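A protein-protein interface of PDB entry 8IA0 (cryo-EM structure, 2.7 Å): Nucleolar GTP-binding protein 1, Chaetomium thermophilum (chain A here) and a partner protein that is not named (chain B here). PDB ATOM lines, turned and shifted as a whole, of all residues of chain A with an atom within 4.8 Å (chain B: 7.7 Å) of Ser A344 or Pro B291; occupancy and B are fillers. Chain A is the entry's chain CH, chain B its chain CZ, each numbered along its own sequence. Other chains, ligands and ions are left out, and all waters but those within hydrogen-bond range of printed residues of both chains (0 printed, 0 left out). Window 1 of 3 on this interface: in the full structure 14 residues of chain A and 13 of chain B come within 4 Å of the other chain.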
ATOM      1  N   VAL A 340     -16.070  15.462   7.108  1.00  0.00           N
ATOM      2  CA  VAL A 340     -14.833  14.728   7.366  1.00  0.00           C
ATOM      3  C   VAL A 340     -14.282  14.139   6.074  1.00  0.00           C
ATOM      4  O   VAL A 340     -13.086  14.250   5.781  1.00  0.00           O
ATOM      5  CB  VAL A 340     -15.070  13.639   8.428  1.00  0.00           C
ATOM      6  CG1 VAL A 340     -13.865  12.720   8.521  1.00  0.00           C
ATOM      7  CG2 VAL A 340     -15.366  14.271   9.773  1.00  0.00           C
ATOM      8  N   GLU A 341     -15.147  13.504   5.281  1.00  0.00           N
ATOM      9  CA  GLU A 341     -14.695  12.890   4.037  1.00  0.00           C
ATOM     10  C   GLU A 341     -14.180  13.935   3.056  1.00  0.00           C
ATOM     11  O   GLU A 341     -13.158  13.723   2.394  1.00  0.00           O
ATOM     12  CB  GLU A 341     -15.829  12.074   3.417  1.00  0.00           C
ATOM     13  CG  GLU A 341     -15.746  11.927   1.907  1.00  0.00           C
ATOM     14  CD  GLU A 341     -16.116  10.534   1.438  1.00  0.00           C
ATOM     15  OE1 GLU A 341     -16.652   9.753   2.252  1.00  0.00           O
ATOM     16  OE2 GLU A 341     -15.871  10.220   0.254  1.00  0.00           O
ATOM     17  N   ARG A 342     -14.874  15.071   2.950  1.00  0.00           N
ATOM     18  CA  ARG A 342     -14.451  16.114   2.021  1.00  0.00           C
ATOM     19  C   ARG A 342     -13.106  16.705   2.422  1.00  0.00           C
ATOM     20  O   ARG A 342     -12.252  16.955   1.565  1.00  0.00           O
ATOM     21  CB  ARG A 342     -15.518  17.205   1.945  1.00  0.00           C
ATOM     22  CG  ARG A 342     -16.700  16.847   1.068  1.00  0.00           C
ATOM     23  CD  ARG A 342     -17.424  18.091   0.604  1.00  0.00           C
ATOM     24  NE  ARG A 342     -17.762  18.039  -0.813  1.00  0.00           N
ATOM     25  CZ  ARG A 342     -17.436  18.978  -1.691  1.00  0.00           C
ATOM     26  NH1 ARG A 342     -16.752  20.052  -1.332  1.00  0.00           N
ATOM     27  NH2 ARG A 342     -17.809  18.837  -2.959  1.00  0.00           N
ATOM     28  N   VAL A 343     -12.901  16.940   3.719  1.00  0.00           N
ATOM     29  CA  VAL A 343     -11.624  17.472   4.184  1.00  0.00           C
ATOM     30  C   VAL A 343     -10.513  16.458   3.950  1.00  0.00           C
ATOM     31  O   VAL A 343      -9.386  16.820   3.590  1.00  0.00           O
ATOM     32  CB  VAL A 343     -11.725  17.884   5.666  1.00  0.00           C
ATOM     33  CG1 VAL A 343     -10.350  18.151   6.247  1.00  0.00           C
ATOM     34  CG2 VAL A 343     -12.603  19.112   5.809  1.00  0.00           C
ATOM     35  N   SER A 344     -10.817  15.173   4.139  1.00  0.00           N
ATOM     36  CA  SER A 344      -9.841  14.129   3.851  1.00  0.00           C
ATOM     37  C   SER A 344      -9.449  14.133   2.381  1.00  0.00           C
ATOM     38  O   SER A 344      -8.270  13.981   2.042  1.00  0.00           O
ATOM     39  CB  SER A 344     -10.405  12.765   4.247  1.00  0.00           C
ATOM     40  OG  SER A 344     -11.003  12.125   3.133  1.00  0.00           O
ATOM     41  N   GLN A 345     -10.429  14.305   1.492  1.00  0.00           N
ATOM     42  CA  GLN A 345     -10.142  14.331   0.063  1.00  0.00           C
ATOM     43  C   GLN A 345      -9.299  15.543  -0.314  1.00  0.00           C
ATOM     44  O   GLN A 345      -8.402  15.444  -1.159  1.00  0.00           O
ATOM     45  CB  GLN A 345     -11.451  14.318  -0.724  1.00  0.00           C
ATOM     46  CG  GLN A 345     -11.896  12.933  -1.157  1.00  0.00           C
ATOM     47  CD  GLN A 345     -12.802  12.965  -2.368  1.00  0.00           C
ATOM     48  OE1 GLN A 345     -13.268  14.027  -2.781  1.00  0.00           O
ATOM     49  NE2 GLN A 345     -13.063  11.797  -2.944  1.00  0.00           N
ATOM     50  N   LYS A 346      -9.580  16.700   0.291  1.00  0.00           N
ATOM     51  CA  LYS A 346      -8.811  17.901  -0.016  1.00  0.00           C
ATOM     52  C   LYS A 346      -7.360  17.755   0.420  1.00  0.00           C
ATOM     53  O   LYS A 346      -6.442  18.162  -0.303  1.00  0.00           O
ATOM     54  CB  LYS A 346      -9.447  19.120   0.650  1.00  0.00           C
ATOM     55  CG  LYS A 346     -10.696  19.623  -0.047  1.00  0.00           C
ATOM     56  CD  LYS A 346     -11.123  20.975   0.488  1.00  0.00           C
ATOM     57  CE  LYS A 346     -12.459  21.392  -0.096  1.00  0.00           C
ATOM     58  NZ  LYS A 346     -12.378  21.614  -1.564  1.00  0.00           N
ATOM     59  N   LEU A 347      -7.131  17.182   1.602  1.00  0.00           N
ATOM     60  CA  LEU A 347      -5.766  16.954   2.061  1.00  0.00           C
ATOM     61  C   LEU A 347      -5.037  15.979   1.146  1.00  0.00           C
ATOM     62  O   LEU A 347      -3.850  16.157   0.854  1.00  0.00           O
ATOM     63  CB  LEU A 347      -5.776  16.438   3.499  1.00  0.00           C
ATOM     64  CG  LEU A 347      -6.215  17.423   4.582  1.00  0.00           C
ATOM     65  CD1 LEU A 347      -6.371  16.716   5.913  1.00  0.00           C
ATOM     66  CD2 LEU A 347      -5.227  18.564   4.704  1.00  0.00           C
ATOM     67  N   LYS A 348      -5.734  14.936   0.688  1.00  0.00           N
ATOM     68  CA  LYS A 348      -5.113  13.953  -0.193  1.00  0.00           C
ATOM     69  C   LYS A 348      -4.684  14.581  -1.511  1.00  0.00           C
ATOM     70  O   LYS A 348      -3.595  14.289  -2.021  1.00  0.00           O
ATOM     71  CB  LYS A 348      -6.077  12.792  -0.440  1.00  0.00           C
ATOM     72  CG  LYS A 348      -5.405  11.433  -0.539  1.00  0.00           C
ATOM     73  CD  LYS A 348      -6.301  10.425  -1.241  1.00  0.00           C
ATOM     74  CE  LYS A 348      -5.483   9.382  -1.986  1.00  0.00           C
ATOM     75  NZ  LYS A 348      -6.186   8.071  -2.056  1.00  0.00           N
ATOM     76  N   TYR B 259      -2.269   5.496   8.869  1.00  0.00           N
ATOM     77  CA  TYR B 259      -3.723   5.424   8.962  1.00  0.00           C
ATOM     78  C   TYR B 259      -4.390   6.412   8.013  1.00  0.00           C
ATOM     79  O   TYR B 259      -5.397   6.087   7.375  1.00  0.00           O
ATOM     80  CB  TYR B 259      -4.175   5.677  10.399  1.00  0.00           C
ATOM     81  CG  TYR B 259      -3.835   4.551  11.346  1.00  0.00           C
ATOM     82  CD1 TYR B 259      -4.329   3.272  11.146  1.00  0.00           C
ATOM     83  CD2 TYR B 259      -3.044   4.778  12.461  1.00  0.00           C
ATOM     84  CE1 TYR B 259      -4.013   2.245  12.013  1.00  0.00           C
ATOM     85  CE2 TYR B 259      -2.729   3.761  13.335  1.00  0.00           C
ATOM     86  CZ  TYR B 259      -3.219   2.496  13.110  1.00  0.00           C
ATOM     87  OH  TYR B 259      -2.911   1.476  13.979  1.00  0.00           O
ATOM     88  N   GLY B 260      -3.850   7.624   7.912  1.00  0.00           N
ATOM     89  CA  GLY B 260      -4.418   8.633   7.054  1.00  0.00           C
ATOM     90  C   GLY B 260      -3.494   9.817   6.865  1.00  0.00           C
ATOM     91  O   GLY B 260      -2.565  10.038   7.648  1.00  0.00           O
ATOM     92  N   PRO B 261      -3.727  10.600   5.808  1.00  0.00           N
ATOM     93  CA  PRO B 261      -2.900  11.796   5.600  1.00  0.00           C
ATOM     94  C   PRO B 261      -3.132  12.892   6.627  1.00  0.00           C
ATOM     95  O   PRO B 261      -2.260  13.752   6.789  1.00  0.00           O
ATOM     96  CB  PRO B 261      -3.281  12.250   4.186  1.00  0.00           C
ATOM     97  CG  PRO B 261      -4.643  11.721   3.970  1.00  0.00           C
ATOM     98  CD  PRO B 261      -4.748  10.439   4.757  1.00  0.00           C
ATOM     99  N   GLU B 262      -4.273  12.899   7.322  1.00  0.00           N
ATOM    100  CA  GLU B 262      -4.467  13.887   8.380  1.00  0.00           C
ATOM    101  C   GLU B 262      -3.440  13.703   9.486  1.00  0.00           C
ATOM    102  O   GLU B 262      -2.876  14.679   9.994  1.00  0.00           O
ATOM    103  CB  GLU B 262      -5.881  13.815   8.978  1.00  0.00           C
ATOM    104  CG  GLU B 262      -7.096  13.743   8.029  1.00  0.00           C
ATOM    105  CD  GLU B 262      -7.075  12.597   7.035  1.00  0.00           C
ATOM    106  OE1 GLU B 262      -6.263  11.665   7.203  1.00  0.00           O
ATOM    107  OE2 GLU B 262      -7.876  12.635   6.080  1.00  0.00           O
ATOM    108  N   LEU B 282     -10.789   5.599  16.811  1.00  0.00           N
ATOM    109  CA  LEU B 282     -12.084   5.695  16.148  1.00  0.00           C
ATOM    110  C   LEU B 282     -13.226   5.740  17.152  1.00  0.00           C
ATOM    111  O   LEU B 282     -14.291   6.290  16.852  1.00  0.00           O
ATOM    112  CB  LEU B 282     -12.276   4.531  15.177  1.00  0.00           C
ATOM    113  CG  LEU B 282     -11.533   4.669  13.849  1.00  0.00           C
ATOM    114  CD1 LEU B 282     -11.823   3.481  12.954  1.00  0.00           C
ATOM    115  CD2 LEU B 282     -11.910   5.968  13.158  1.00  0.00           C
ATOM    116  N   PRO B 286     -15.885   8.731  15.908  1.00  0.00           N
ATOM    117  CA  PRO B 286     -16.457   7.712  15.010  1.00  0.00           C
ATOM    118  C   PRO B 286     -16.566   8.148  13.560  1.00  0.00           C
ATOM    119  O   PRO B 286     -16.640   7.284  12.678  1.00  0.00           O
ATOM    120  CB  PRO B 286     -17.847   7.438  15.604  1.00  0.00           C
ATOM    121  CG  PRO B 286     -17.891   8.103  16.924  1.00  0.00           C
ATOM    122  CD  PRO B 286     -16.733   9.025  17.075  1.00  0.00           C
ATOM    123  N   SER B 287     -16.578   9.451  13.278  1.00  0.00           N
ATOM    124  CA  SER B 287     -16.804   9.930  11.920  1.00  0.00           C
ATOM    125  C   SER B 287     -15.639   9.655  10.977  1.00  0.00           C
ATOM    126  O   SER B 287     -15.808   9.794   9.761  1.00  0.00           O
ATOM    127  CB  SER B 287     -17.104  11.431  11.933  1.00  0.00           C
ATOM    128  OG  SER B 287     -18.275  11.709  12.680  1.00  0.00           O
ATOM    129  N   LYS B 288     -14.472   9.272  11.491  1.00  0.00           N
ATOM    130  CA  LYS B 288     -13.326   8.971  10.647  1.00  0.00           C
ATOM    131  C   LYS B 288     -13.237   7.501  10.263  1.00  0.00           C
ATOM    132  O   LYS B 288     -12.214   7.083   9.711  1.00  0.00           O
ATOM    133  CB  LYS B 288     -12.022   9.391  11.332  1.00  0.00           C
ATOM    134  CG  LYS B 288     -12.115  10.661  12.150  1.00  0.00           C
ATOM    135  CD  LYS B 288     -10.971  10.750  13.146  1.00  0.00           C
ATOM    136  CE  LYS B 288      -9.723  11.335  12.507  1.00  0.00           C
ATOM    137  NZ  LYS B 288      -9.998  12.639  11.846  1.00  0.00           N
ATOM    138  N   ARG B 289     -14.272   6.707  10.548  1.00  0.00           N
ATOM    139  CA  ARG B 289     -14.226   5.286  10.221  1.00  0.00           C
ATOM    140  C   ARG B 289     -14.084   5.068   8.721  1.00  0.00           C
ATOM    141  O   ARG B 289     -13.213   4.317   8.270  1.00  0.00           O
ATOM    142  CB  ARG B 289     -15.479   4.586  10.748  1.00  0.00           C
ATOM    143  CG  ARG B 289     -15.212   3.582  11.853  1.00  0.00           C
ATOM    144  CD  ARG B 289     -16.346   2.584  11.988  1.00  0.00           C
ATOM    145  NE  ARG B 289     -16.419   1.686  10.842  1.00  0.00           N
ATOM    146  CZ  ARG B 289     -15.854   0.488  10.792  1.00  0.00           C
ATOM    147  NH1 ARG B 289     -15.152   0.012  11.807  1.00  0.00           N
ATOM    148  NH2 ARG B 289     -15.996  -0.251   9.696  1.00  0.00           N
ATOM    149  N   ALA B 290     -14.936   5.719   7.930  1.00  0.00           N
ATOM    150  CA  ALA B 290     -14.932   5.490   6.487  1.00  0.00           C
ATOM    151  C   ALA B 290     -13.640   5.926   5.806  1.00  0.00           C
ATOM    152  O   ALA B 290     -13.070   5.121   5.050  1.00  0.00           O
ATOM    153  CB  ALA B 290     -16.152   6.168   5.857  1.00  0.00           C
ATOM    154  N   PRO B 291     -13.123   7.146   6.005  1.00  0.00           N
ATOM    155  CA  PRO B 291     -11.940   7.547   5.224  1.00  0.00           C
ATOM    156  C   PRO B 291     -10.666   6.838   5.644  1.00  0.00           C
ATOM    157  O   PRO B 291      -9.834   6.512   4.788  1.00  0.00           O
ATOM    158  CB  PRO B 291     -11.850   9.062   5.473  1.00  0.00           C
ATOM    159  CG  PRO B 291     -13.161   9.448   6.083  1.00  0.00           C
ATOM    160  CD  PRO B 291     -13.593   8.253   6.853  1.00  0.00           C
ATOM    161  N   VAL B 292     -10.486   6.594   6.944  1.00  0.00           N
ATOM    162  CA  VAL B 292      -9.249   5.982   7.424  1.00  0.00           C
ATOM    163  C   VAL B 292      -9.115   4.563   6.886  1.00  0.00           C
ATOM    164  O   VAL B 292      -8.037   4.145   6.447  1.00  0.00           O
ATOM    165  CB  VAL B 292      -9.198   6.012   8.961  1.00  0.00           C
ATOM    166  CG1 VAL B 292      -8.165   5.028   9.481  1.00  0.00           C
ATOM    167  CG2 VAL B 292      -8.895   7.419   9.451  1.00  0.00           C
ATOM    168  N   LEU B 293     -10.211   3.803   6.909  1.00  0.00           N
ATOM    169  CA  LEU B 293     -10.165   2.428   6.425  1.00  0.00           C
ATOM    170  C   LEU B 293      -9.856   2.377   4.935  1.00  0.00           C
ATOM    171  O   LEU B 293      -9.097   1.513   4.482  1.00  0.00           O
ATOM    172  CB  LEU B 293     -11.485   1.722   6.726  1.00  0.00           C
ATOM    173  CG  LEU B 293     -11.757   1.456   8.206  1.00  0.00           C
ATOM    174  CD1 LEU B 293     -13.096   0.761   8.389  1.00  0.00           C
ATOM    175  CD2 LEU B 293     -10.636   0.635   8.821  1.00  0.00           C
ATOM    176  N   LYS B 294     -10.438   3.289   4.158  1.00  0.00           N
ATOM    177  CA  LYS B 294     -10.156   3.329   2.727  1.00  0.00           C
ATOM    178  C   LYS B 294      -8.689   3.644   2.469  1.00  0.00           C
ATOM    179  O   LYS B 294      -8.052   3.028   1.607  1.00  0.00           O
ATOM    180  CB  LYS B 294     -11.062   4.355   2.046  1.00  0.00           C
ATOM    181  CG  LYS B 294     -10.636   4.719   0.632  1.00  0.00           C
ATOM    182  CD  LYS B 294     -11.609   5.698  -0.012  1.00  0.00           C
ATOM    183  CE  LYS B 294     -13.020   5.132  -0.100  1.00  0.00           C
ATOM    184  NZ  LYS B 294     -13.043   3.665  -0.370  1.00  0.00           N
ATOM    185  N   TYR B 295      -8.133   4.607   3.207  1.00  0.00           N
ATOM    186  CA  TYR B 295      -6.718   4.931   3.053  1.00  0.00           C
ATOM    187  C   TYR B 295      -5.840   3.766   3.485  1.00  0.00           C
ATOM    188  O   TYR B 295      -4.844   3.444   2.826  1.00  0.00           O
ATOM    189  CB  TYR B 295      -6.370   6.185   3.852  1.00  0.00           C
ATOM    190  CG  TYR B 295      -5.138   6.897   3.349  1.00  0.00           C
ATOM    191  CD1 TYR B 295      -5.136   7.537   2.119  1.00  0.00           C
ATOM    192  CD2 TYR B 295      -3.970   6.913   4.095  1.00  0.00           C
ATOM    193  CE1 TYR B 295      -4.009   8.185   1.653  1.00  0.00           C
ATOM    194  CE2 TYR B 295      -2.839   7.558   3.640  1.00  0.00           C
ATOM    195  CZ  TYR B 295      -2.863   8.191   2.418  1.00  0.00           C
ATOM    196  OH  TYR B 295      -1.737   8.834   1.958  1.00  0.00           O
ATOM    197  N   LEU B 296      -6.190   3.125   4.601  1.00  0.00           N
ATOM    198  CA  LEU B 296      -5.404   1.993   5.077  1.00  0.00           C
ATOM    199  C   LEU B 296      -5.464   0.829   4.098  1.00  0.00           C
ATOM    200  O   LEU B 296      -4.450   0.169   3.844  1.00  0.00           O
ATOM    201  CB  LEU B 296      -5.891   1.561   6.459  1.00  0.00           C
ATOM    202  CG  LEU B 296      -4.933   0.688   7.267  1.00  0.00           C
ATOM    203  CD1 LEU B 296      -3.502   1.175   7.117  1.00  0.00           C
ATOM    204  CD2 LEU B 296      -5.341   0.667   8.728  1.00  0.00           C
ATOM    205  N   PHE B 297      -6.646   0.559   3.539  1.00  0.00           N
ATOM    206  CA  PHE B 297      -6.775  -0.533   2.579  1.00  0.00           C
ATOM    207  C   PHE B 297      -6.000  -0.246   1.302  1.00  0.00           C
ATOM    208  O   PHE B 297      -5.319  -1.130   0.773  1.00  0.00           O
ATOM    209  CB  PHE B 297      -8.246  -0.783   2.255  1.00  0.00           C
ATOM    210  CG  PHE B 297      -8.478  -1.981   1.380  1.00  0.00           C
ATOM    211  CD1 PHE B 297      -8.247  -3.257   1.861  1.00  0.00           C
ATOM    212  CD2 PHE B 297      -8.937  -1.832   0.085  1.00  0.00           C
ATOM    213  CE1 PHE B 297      -8.463  -4.361   1.065  1.00  0.00           C
ATOM    214  CE2 PHE B 297      -9.156  -2.934  -0.717  1.00  0.00           C
ATOM    215  CZ  PHE B 297      -8.918  -4.201  -0.226  1.00  0.00           C
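Printed residues of chain B within 4 Å of Val A340: Ser B287. Of chain B, only Glu B262 and Pro B291 come within 4 Å of Ser A344. Of the printed residues of chain B, Leu A347 touches Glu B262 (3.7 Å). Lys A348 touches none of the printed residues of chain B. Of the printed residues of chain A, Glu B262 touches Ser A344 (3.1 Å) and Leu A347 (3.7 Å). Of the printed residues of chain A, Ser B287 touches Val A340. Printed residues of chain A within 4 Å of Pro B291: Ser A344 (3.9 Å). The nearest residue of chain A that does not touch Pro B291 is Val A340 (4.1 Å). The nearest printed residue of chain B that does not touch Leu A347 is Pro B261 (4.9 Å).
Val A340 touches Ser B287 (CG1 to O, 3.7 Å). Ser A344 touches Glu B262. Ser A344 touches Pro B291. CD1 of Leu A347 touches CG of Glu B262, 3.7 Å away.
The backbone carbonyl oxygen (O) of Glu A341 is in hydrogen-bond range of the side-chain hydroxyl (OG) of Ser A344 (2.8 Å).
Hydrophobic or aromatic side chains of chain A that line the printed part of chain B: Val A340 and Leu A347. Of the 17 printed residues of chain B, 3 touch a printed residue of chain A. Hydrophobic or aromatic side chains of chain B that line the printed part of chain A: Pro B291. Among the printed residues, no Asp or Glu carboxylate lies within 4 Å of a Lys or Arg side-chain nitrogen of the other chain.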
